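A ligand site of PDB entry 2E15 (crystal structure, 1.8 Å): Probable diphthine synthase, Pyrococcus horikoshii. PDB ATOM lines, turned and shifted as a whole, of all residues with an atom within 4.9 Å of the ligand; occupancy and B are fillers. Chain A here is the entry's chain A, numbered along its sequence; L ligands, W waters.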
ATOM      1  N   LEU A  10      -7.714 -15.465  -9.069  1.00  0.00           N
ATOM      2  CA  LEU A  10      -7.644 -14.073  -8.653  1.00  0.00           C
ATOM      3  C   LEU A  10      -8.026 -12.899  -9.541  1.00  0.00           C
ATOM      4  O   LEU A  10      -8.694 -11.971  -9.077  1.00  0.00           O
ATOM      5  CB  LEU A  10      -6.219 -13.788  -8.176  1.00  0.00           C
ATOM      6  CG  LEU A  10      -5.617 -14.714  -7.130  1.00  0.00           C
ATOM      7  CD1 LEU A  10      -4.111 -14.525  -7.087  1.00  0.00           C
ATOM      8  CD2 LEU A  10      -6.234 -14.427  -5.776  1.00  0.00           C
ATOM      9  N   TYR A  11      -7.616 -12.934 -10.795  1.00  0.00           N
ATOM     10  CA  TYR A  11      -7.818 -11.772 -11.646  1.00  0.00           C
ATOM     11  C   TYR A  11      -8.461 -11.940 -13.023  1.00  0.00           C
ATOM     12  O   TYR A  11      -9.384 -11.213 -13.361  1.00  0.00           O
ATOM     13  CB  TYR A  11      -6.448 -11.093 -11.791  1.00  0.00           C
ATOM     14  CG  TYR A  11      -6.434  -9.792 -12.552  1.00  0.00           C
ATOM     15  CD1 TYR A  11      -7.008  -8.647 -12.005  1.00  0.00           C
ATOM     16  CD2 TYR A  11      -5.807  -9.705 -13.784  1.00  0.00           C
ATOM     17  CE1 TYR A  11      -6.940  -7.428 -12.685  1.00  0.00           C
ATOM     18  CE2 TYR A  11      -5.731  -8.495 -14.472  1.00  0.00           C
ATOM     19  CZ  TYR A  11      -6.306  -7.362 -13.913  1.00  0.00           C
ATOM     20  OH  TYR A  11      -6.224  -6.171 -14.588  1.00  0.00           O
ATOM     21  N   THR A  36     -19.209 -13.278  -4.776  1.00  0.00           N
ATOM     22  CA  THR A  36     -18.327 -13.464  -3.623  1.00  0.00           C
ATOM     23  C   THR A  36     -17.022 -12.693  -3.769  1.00  0.00           C
ATOM     24  O   THR A  36     -16.356 -12.393  -2.785  1.00  0.00           O
ATOM     25  CB  THR A  36     -18.006 -14.948  -3.383  1.00  0.00           C
ATOM     26  OG1 THR A  36     -17.409 -15.511  -4.569  1.00  0.00           O
ATOM     27  CG2 THR A  36     -19.258 -15.716  -3.046  1.00  0.00           C
ATOM     28  N   SER A  37     -16.646 -12.382  -5.005  1.00  0.00           N
ATOM     29  CA  SER A  37     -15.414 -11.636  -5.239  1.00  0.00           C
ATOM     30  C   SER A  37     -15.428 -10.991  -6.615  1.00  0.00           C
ATOM     31  O   SER A  37     -16.340 -11.227  -7.417  1.00  0.00           O
ATOM     32  CB  SER A  37     -14.205 -12.553  -5.112  1.00  0.00           C
ATOM     33  OG  SER A  37     -13.020 -11.787  -5.100  1.00  0.00           O
ATOM     34  N   LEU A  38     -14.419 -10.178  -6.898  1.00  0.00           N
ATOM     35  CA  LEU A  38     -14.318  -9.491  -8.172  1.00  0.00           C
ATOM     36  C   LEU A  38     -13.082  -9.900  -8.968  1.00  0.00           C
ATOM     37  O   LEU A  38     -11.958  -9.794  -8.465  1.00  0.00           O
ATOM     38  CB  LEU A  38     -14.285  -7.977  -7.962  1.00  0.00           C
ATOM     39  CG  LEU A  38     -14.040  -7.110  -9.211  1.00  0.00           C
ATOM     40  CD1 LEU A  38     -15.225  -7.228 -10.158  1.00  0.00           C
ATOM     41  CD2 LEU A  38     -13.819  -5.658  -8.804  1.00  0.00           C
ATOM     42  N   PRO A  85     -15.086 -17.169  -8.262  1.00  0.00           N
ATOM     43  CA  PRO A  85     -13.821 -16.413  -8.320  1.00  0.00           C
ATOM     44  C   PRO A  85     -12.920 -16.987  -7.233  1.00  0.00           C
ATOM     45  O   PRO A  85     -13.416 -17.590  -6.268  1.00  0.00           O
ATOM     46  CB  PRO A  85     -14.261 -14.991  -7.987  1.00  0.00           C
ATOM     47  CG  PRO A  85     -15.681 -14.942  -8.470  1.00  0.00           C
ATOM     48  CD  PRO A  85     -16.223 -16.266  -8.022  1.00  0.00           C
ATOM     49  N   GLY A  86     -11.611 -16.800  -7.379  1.00  0.00           N
ATOM     50  CA  GLY A  86     -10.669 -17.302  -6.388  1.00  0.00           C
ATOM     51  C   GLY A  86     -10.819 -18.795  -6.148  1.00  0.00           C
ATOM     52  O   GLY A  86     -11.010 -19.558  -7.086  1.00  0.00           O
ATOM     53  N   ASP A  87     -10.706 -19.200  -4.885  1.00  0.00           N
ATOM     54  CA  ASP A  87     -10.875 -20.602  -4.508  1.00  0.00           C
ATOM     55  C   ASP A  87     -12.338 -20.690  -4.071  1.00  0.00           C
ATOM     56  O   ASP A  87     -12.799 -19.855  -3.282  1.00  0.00           O
ATOM     57  CB  ASP A  87      -9.932 -20.977  -3.372  1.00  0.00           C
ATOM     58  CG  ASP A  87     -10.102 -22.420  -2.928  1.00  0.00           C
ATOM     59  OD1 ASP A  87     -11.185 -22.761  -2.384  1.00  0.00           O
ATOM     60  OD2 ASP A  87      -9.164 -23.222  -3.128  1.00  0.00           O
ATOM     61  N   VAL A  90     -12.986 -20.600  -0.015  1.00  0.00           N
ATOM     62  CA  VAL A  90     -12.317 -19.638   0.858  1.00  0.00           C
ATOM     63  C   VAL A  90     -13.127 -18.356   1.028  1.00  0.00           C
ATOM     64  O   VAL A  90     -13.446 -17.672   0.065  1.00  0.00           O
ATOM     65  CB  VAL A  90     -10.926 -19.239   0.296  1.00  0.00           C
ATOM     66  CG1 VAL A  90     -10.320 -18.128   1.149  1.00  0.00           C
ATOM     67  CG2 VAL A  90     -10.014 -20.453   0.262  1.00  0.00           C
ATOM     68  N   ALA A  91     -13.459 -18.030   2.272  1.00  0.00           N
ATOM     69  CA  ALA A  91     -14.221 -16.824   2.572  1.00  0.00           C
ATOM     70  C   ALA A  91     -15.568 -16.764   1.863  1.00  0.00           C
ATOM     71  O   ALA A  91     -16.073 -15.691   1.524  1.00  0.00           O
ATOM     72  CB  ALA A  91     -13.386 -15.581   2.235  1.00  0.00           C
ATOM     73  N   THR A  92     -16.134 -17.940   1.626  1.00  0.00           N
ATOM     74  CA  THR A  92     -17.477 -18.124   1.114  1.00  0.00           C
ATOM     75  C   THR A  92     -18.224 -19.098   2.006  1.00  0.00           C
ATOM     76  O   THR A  92     -17.664 -19.700   2.919  1.00  0.00           O
ATOM     77  CB  THR A  92     -17.390 -18.686  -0.313  1.00  0.00           C
ATOM     78  OG1 THR A  92     -17.082 -20.087  -0.249  1.00  0.00           O
ATOM     79  CG2 THR A  92     -16.283 -17.973  -1.109  1.00  0.00           C
ATOM     80  N   PRO A 114      -5.913 -20.172  -7.294  1.00  0.00           N
ATOM     81  CA  PRO A 114      -5.235 -19.190  -6.433  1.00  0.00           C
ATOM     82  C   PRO A 114      -6.244 -18.344  -5.658  1.00  0.00           C
ATOM     83  O   PRO A 114      -7.244 -17.880  -6.204  1.00  0.00           O
ATOM     84  CB  PRO A 114      -4.383 -18.378  -7.410  1.00  0.00           C
ATOM     85  CG  PRO A 114      -4.970 -18.674  -8.772  1.00  0.00           C
ATOM     86  CD  PRO A 114      -5.408 -20.104  -8.672  1.00  0.00           C
ATOM     87  N   SER A 115      -5.960 -18.169  -4.371  1.00  0.00           N
ATOM     88  CA  SER A 115      -6.834 -17.428  -3.472  1.00  0.00           C
ATOM     89  C   SER A 115      -6.121 -16.214  -2.894  1.00  0.00           C
ATOM     90  O   SER A 115      -4.912 -16.236  -2.698  1.00  0.00           O
ATOM     91  CB  SER A 115      -7.281 -18.334  -2.315  1.00  0.00           C
ATOM     92  OG  SER A 115      -7.961 -17.589  -1.319  1.00  0.00           O
ATOM     93  N   ILE A 116      -6.873 -15.159  -2.602  1.00  0.00           N
ATOM     94  CA  ILE A 116      -6.251 -13.967  -2.033  1.00  0.00           C
ATOM     95  C   ILE A 116      -5.668 -14.305  -0.665  1.00  0.00           C
ATOM     96  O   ILE A 116      -4.697 -13.691  -0.223  1.00  0.00           O
ATOM     97  CB  ILE A 116      -7.277 -12.822  -1.893  1.00  0.00           C
ATOM     98  CG1 ILE A 116      -6.558 -11.543  -1.466  1.00  0.00           C
ATOM     99  CG2 ILE A 116      -8.338 -13.197  -0.873  1.00  0.00           C
ATOM    100  CD1 ILE A 116      -5.523 -11.057  -2.464  1.00  0.00           C
ATOM    101  N   TYR A 117      -6.257 -15.298   0.006  1.00  0.00           N
ATOM    102  CA  TYR A 117      -5.796 -15.712   1.337  1.00  0.00           C
ATOM    103  C   TYR A 117      -4.318 -16.106   1.347  1.00  0.00           C
ATOM    104  O   TYR A 117      -3.615 -15.857   2.323  1.00  0.00           O
ATOM    105  CB  TYR A 117      -6.682 -16.861   1.837  1.00  0.00           C
ATOM    106  CG  TYR A 117      -6.374 -17.348   3.241  1.00  0.00           C
ATOM    107  CD1 TYR A 117      -6.563 -16.529   4.353  1.00  0.00           C
ATOM    108  CD2 TYR A 117      -5.944 -18.658   3.461  1.00  0.00           C
ATOM    109  CE1 TYR A 117      -6.339 -17.003   5.642  1.00  0.00           C
ATOM    110  CE2 TYR A 117      -5.712 -19.140   4.741  1.00  0.00           C
ATOM    111  CZ  TYR A 117      -5.913 -18.309   5.830  1.00  0.00           C
ATOM    112  OH  TYR A 117      -5.693 -18.793   7.099  1.00  0.00           O
ATOM    113  N   PHE A 165     -10.456  -8.817   4.618  1.00  0.00           N
ATOM    114  CA  PHE A 165     -11.188  -8.937   3.375  1.00  0.00           C
ATOM    115  C   PHE A 165     -12.059  -7.679   3.368  1.00  0.00           C
ATOM    116  O   PHE A 165     -12.511  -7.249   4.429  1.00  0.00           O
ATOM    117  CB  PHE A 165     -12.112 -10.164   3.412  1.00  0.00           C
ATOM    118  CG  PHE A 165     -11.378 -11.468   3.438  1.00  0.00           C
ATOM    119  CD1 PHE A 165     -10.862 -12.021   2.271  1.00  0.00           C
ATOM    120  CD2 PHE A 165     -11.219 -12.161   4.636  1.00  0.00           C
ATOM    121  CE1 PHE A 165     -10.186 -13.238   2.297  1.00  0.00           C
ATOM    122  CE2 PHE A 165     -10.538 -13.384   4.674  1.00  0.00           C
ATOM    123  CZ  PHE A 165     -10.020 -13.924   3.495  1.00  0.00           C
ATOM    124  N   LEU A 166     -12.273  -7.088   2.207  1.00  0.00           N
ATOM    125  CA  LEU A 166     -13.090  -5.884   2.123  1.00  0.00           C
ATOM    126  C   LEU A 166     -14.458  -6.199   1.535  1.00  0.00           C
ATOM    127  O   LEU A 166     -14.591  -7.105   0.707  1.00  0.00           O
ATOM    128  CB  LEU A 166     -12.369  -4.813   1.306  1.00  0.00           C
ATOM    129  CG  LEU A 166     -10.966  -4.476   1.845  1.00  0.00           C
ATOM    130  CD1 LEU A 166     -10.407  -3.269   1.120  1.00  0.00           C
ATOM    131  CD2 LEU A 166     -11.047  -4.203   3.344  1.00  0.00           C
ATOM    132  N   ASP A 167     -15.477  -5.471   1.969  1.00  0.00           N
ATOM    133  CA  ASP A 167     -16.843  -5.717   1.524  1.00  0.00           C
ATOM    134  C   ASP A 167     -17.064  -5.587   0.020  1.00  0.00           C
ATOM    135  O   ASP A 167     -16.318  -4.908  -0.688  1.00  0.00           O
ATOM    136  CB  ASP A 167     -17.818  -4.776   2.260  1.00  0.00           C
ATOM    137  CG  ASP A 167     -19.188  -5.397   2.458  1.00  0.00           C
ATOM    138  OD1 ASP A 167     -19.429  -6.504   1.919  1.00  0.00           O
ATOM    139  OD2 ASP A 167     -20.015  -4.790   3.169  1.00  0.00           O
ATOM    140  N   ILE A 168     -18.103  -6.260  -0.443  1.00  0.00           N
ATOM    141  CA  ILE A 168     -18.472  -6.250  -1.849  1.00  0.00           C
ATOM    142  C   ILE A 168     -19.988  -6.358  -1.976  1.00  0.00           C
ATOM    143  O   ILE A 168     -20.633  -7.138  -1.271  1.00  0.00           O
ATOM    144  CB  ILE A 168     -17.806  -7.420  -2.615  1.00  0.00           C
ATOM    145  CG1 ILE A 168     -18.365  -7.503  -4.033  1.00  0.00           C
ATOM    146  CG2 ILE A 168     -18.017  -8.735  -1.868  1.00  0.00           C
ATOM    147  CD1 ILE A 168     -17.720  -8.580  -4.906  1.00  0.00           C
ATOM    148  N   LEU A 206      -2.935  -4.393  -0.878  1.00  0.00           N
ATOM    149  CA  LEU A 206      -2.681  -5.234  -2.040  1.00  0.00           C
ATOM    150  C   LEU A 206      -3.904  -5.102  -2.936  1.00  0.00           C
ATOM    151  O   LEU A 206      -5.011  -5.448  -2.537  1.00  0.00           O
ATOM    152  CB  LEU A 206      -2.489  -6.701  -1.636  1.00  0.00           C
ATOM    153  CG  LEU A 206      -2.303  -7.674  -2.820  1.00  0.00           C
ATOM    154  CD1 LEU A 206      -1.090  -7.267  -3.651  1.00  0.00           C
ATOM    155  CD2 LEU A 206      -2.128  -9.095  -2.293  1.00  0.00           C
ATOM    156  N   ALA A 207      -3.705  -4.556  -4.137  1.00  0.00           N
ATOM    157  CA  ALA A 207      -4.811  -4.370  -5.054  1.00  0.00           C
ATOM    158  C   ALA A 207      -4.612  -5.143  -6.346  1.00  0.00           C
ATOM    159  O   ALA A 207      -3.528  -5.116  -6.937  1.00  0.00           O
ATOM    160  CB  ALA A 207      -4.988  -2.875  -5.358  1.00  0.00           C
ATOM    161  N   ARG A 208      -5.664  -5.832  -6.768  1.00  0.00           N
ATOM    162  CA  ARG A 208      -5.666  -6.630  -7.991  1.00  0.00           C
ATOM    163  C   ARG A 208      -4.593  -7.708  -8.012  1.00  0.00           C
ATOM    164  O   ARG A 208      -3.835  -7.851  -8.980  1.00  0.00           O
ATOM    165  CB  ARG A 208      -5.518  -5.693  -9.212  1.00  0.00           C
ATOM    166  CG  ARG A 208      -6.637  -4.654  -9.324  1.00  0.00           C
ATOM    167  CD  ARG A 208      -6.400  -3.722 -10.512  1.00  0.00           C
ATOM    168  NE  ARG A 208      -5.044  -3.184 -10.487  1.00  0.00           N
ATOM    169  CZ  ARG A 208      -4.598  -2.296  -9.604  1.00  0.00           C
ATOM    170  NH1 ARG A 208      -5.405  -1.820  -8.658  1.00  0.00           N
ATOM    171  NH2 ARG A 208      -3.332  -1.910  -9.651  1.00  0.00           N
ATOM    172  N   ALA A 209      -4.531  -8.488  -6.937  1.00  0.00           N
ATOM    173  CA  ALA A 209      -3.583  -9.582  -6.871  1.00  0.00           C
ATOM    174  C   ALA A 209      -3.965 -10.494  -8.027  1.00  0.00           C
ATOM    175  O   ALA A 209      -5.138 -10.593  -8.375  1.00  0.00           O
ATOM    176  CB  ALA A 209      -3.719 -10.332  -5.542  1.00  0.00           C
ATOM    177  N   GLY A 210      -2.980 -11.147  -8.639  1.00  0.00           N
ATOM    178  CA  GLY A 210      -3.281 -12.012  -9.761  1.00  0.00           C
ATOM    179  C   GLY A 210      -2.875 -11.363 -11.070  1.00  0.00           C
ATOM    180  O   GLY A 210      -2.480 -12.034 -12.024  1.00  0.00           O
ATOM    181  N   PRO A 233     -10.383  -5.288  -7.090  1.00  0.00           N
ATOM    182  CA  PRO A 233     -10.561  -5.400  -5.642  1.00  0.00           C
ATOM    183  C   PRO A 233      -9.308  -5.054  -4.840  1.00  0.00           C
ATOM    184  O   PRO A 233      -8.176  -5.116  -5.351  1.00  0.00           O
ATOM    185  CB  PRO A 233     -10.981  -6.849  -5.465  1.00  0.00           C
ATOM    186  CG  PRO A 233     -10.152  -7.545  -6.510  1.00  0.00           C
ATOM    187  CD  PRO A 233     -10.283  -6.625  -7.715  1.00  0.00           C
ATOM    188  N   HIS A 234      -9.513  -4.685  -3.584  1.00  0.00           N
ATOM    189  CA  HIS A 234      -8.432  -4.336  -2.673  1.00  0.00           C
ATOM    190  C   HIS A 234      -8.549  -5.191  -1.428  1.00  0.00           C
ATOM    191  O   HIS A 234      -9.640  -5.652  -1.083  1.00  0.00           O
ATOM    192  CB  HIS A 234      -8.551  -2.881  -2.179  1.00  0.00           C
ATOM    193  CG  HIS A 234      -8.387  -1.846  -3.249  1.00  0.00           C
ATOM    194  ND1 HIS A 234      -8.434  -0.493  -2.966  1.00  0.00           N
ATOM    195  CD2 HIS A 234      -8.180  -1.947  -4.582  1.00  0.00           C
ATOM    196  CE1 HIS A 234      -8.263   0.194  -4.077  1.00  0.00           C
ATOM    197  NE2 HIS A 234      -8.102  -0.667  -5.076  1.00  0.00           N
ATOM    198  N   ILE A 235      -7.432  -5.388  -0.752  1.00  0.00           N
ATOM    199  CA  ILE A 235      -7.439  -6.084   0.516  1.00  0.00           C
ATOM    200  C   ILE A 235      -6.536  -5.243   1.406  1.00  0.00           C
ATOM    201  O   ILE A 235      -5.578  -4.634   0.930  1.00  0.00           O
ATOM    202  CB  ILE A 235      -6.940  -7.550   0.380  1.00  0.00           C
ATOM    203  CG1 ILE A 235      -7.415  -8.357   1.580  1.00  0.00           C
ATOM    204  CG2 ILE A 235      -5.427  -7.596   0.274  1.00  0.00           C
ATOM    205  CD1 ILE A 235      -7.676  -9.812   1.259  1.00  0.00           C
HETATM  206  N1  LIG L   1     -12.903 -17.138  -2.433  1.00  0.00           N
HETATM  207  C1  LIG L   1     -12.190 -15.814  -2.715  1.00  0.00           C
HETATM  208  C2  LIG L   1     -12.378 -14.713  -1.733  1.00  0.00           C
HETATM  209  C3  LIG L   1     -13.792 -14.226  -1.431  1.00  0.00           C
HETATM  210  S1  LIG L   1     -13.618 -12.751  -0.350  1.00  0.00           S
HETATM  211  C4  LIG L   1     -10.654 -16.166  -2.867  1.00  0.00           C
HETATM  212  O1  LIG L   1     -10.294 -17.350  -2.725  1.00  0.00           O
HETATM  213  O2  LIG L   1      -9.861 -15.178  -3.143  1.00  0.00           O
HETATM  214  C5  LIG L   1     -13.565 -11.492  -1.568  1.00  0.00           C
HETATM  215  C6  LIG L   1     -12.669 -10.292  -1.076  1.00  0.00           C
HETATM  216  O3  LIG L   1     -11.282 -10.750  -1.070  1.00  0.00           O
HETATM  217  C7  LIG L   1     -12.704  -9.084  -1.942  1.00  0.00           C
HETATM  218  O4  LIG L   1     -13.776  -8.217  -1.545  1.00  0.00           O
HETATM  219  C8  LIG L   1     -11.280  -8.501  -1.740  1.00  0.00           C
HETATM  220  O5  LIG L   1     -11.194  -7.703  -0.557  1.00  0.00           O
HETATM  221  C9  LIG L   1     -10.378  -9.748  -1.700  1.00  0.00           C
HETATM  222  N2  LIG L   1      -9.936 -10.183  -2.904  1.00  0.00           N
HETATM  223  C10 LIG L   1     -10.306 -11.191  -3.770  1.00  0.00           C
HETATM  224  N3  LIG L   1      -9.604 -11.277  -4.855  1.00  0.00           N
HETATM  225  C11 LIG L   1      -8.642 -10.230  -4.740  1.00  0.00           C
HETATM  226  C12 LIG L   1      -7.580  -9.799  -5.615  1.00  0.00           C
HETATM  227  N4  LIG L   1      -7.298 -10.372  -6.791  1.00  0.00           N
HETATM  228  N5  LIG L   1      -6.856  -8.723  -5.159  1.00  0.00           N
HETATM  229  C13 LIG L   1      -7.104  -8.100  -3.976  1.00  0.00           C
HETATM  230  N6  LIG L   1      -8.109  -8.490  -3.109  1.00  0.00           N
HETATM  231  C14 LIG L   1      -8.833  -9.551  -3.557  1.00  0.00           C
HETATM  232  O   HOH W   1     -14.802 -16.258  -4.175  1.00  0.00           O
HETATM  233  O   HOH W   2     -14.529  -5.795  -2.931  1.00  0.00           O
HETATM  234  O   HOH W   3     -11.345 -12.701  -7.396  1.00  0.00           O
HETATM  235  O   HOH W   4     -10.059 -14.014  -5.685  1.00  0.00           O
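A sulfur (S1) of the ligand lies close to the backbone carbonyl oxygen (O) of Thr 36 (3.7 Å). Merely in contact with the ligand: Pro 233, Arg 208, Phe 165, Leu 206, Gly 86, Thr 92, Ile 235, Ala 91 and Pro 85. The nearest printed residue that does not touch the ligand is Ile 168 (4.2 Å).
OG of Ser 115 lies close to N of Tyr 117 (3.1 Å). O of Pro 233 is in hydrogen-bond range of N of Arg 208. N of Ile 235 lies within hydrogen-bond range of O of Leu 206, 3.0 Å away.
Water W1 lies within hydrogen-bond range of a nitrogen (N1) of the ligand (2.7 Å), the side-chain hydroxyl (OG1) of Thr 36 (2.7 Å) and the backbone carbonyl oxygen (O) of Pro 85 (2.8 Å). Water W2 bridges O4 of the ligand (2.9 Å) and O of Asp 167 (3.0 Å).
The backbone carbonyl oxygen of Val 90 is in hydrogen-bond range of a nitrogen (N1) of the ligand (2.6 Å). O of His 234 lies within hydrogen-bond range of O5 of the ligand. The backbone NH (N) of Leu 166 lies within hydrogen-bond range of an oxygen (O5) of the ligand (3.0 Å). An oxygen (O4) of the ligand sits at hydrogen-bond distance from the backbone carbonyl oxygen (O) of Leu 166, at 2.6 Å. The backbone NH (N) of Ala 209 sits at hydrogen-bond distance from a nitrogen (N5) of the ligand. The backbone carbonyl oxygen (O) of Ala 209 sits at hydrogen-bond distance from a nitrogen (N4) of the ligand (2.7 Å). The side-chain hydroxyl (OG) of Ser 115 is in hydrogen-bond range of an oxygen (O1) of the ligand (2.7 Å). N of Asp 87 is in hydrogen-bond range of O1 of the ligand (2.9 Å). The backbone carbonyl oxygen (O) of Asp 87 is in hydrogen-bond range of a nitrogen (N1) of the ligand (2.8 Å). O2 of the ligand is in hydrogen-bond range of N of Ile 116 (3.0 Å). N3 of the ligand lies close to OG of Ser 37. A nitrogen (N4) of the ligand lies within hydrogen-bond range of the backbone carbonyl oxygen of Leu 10.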
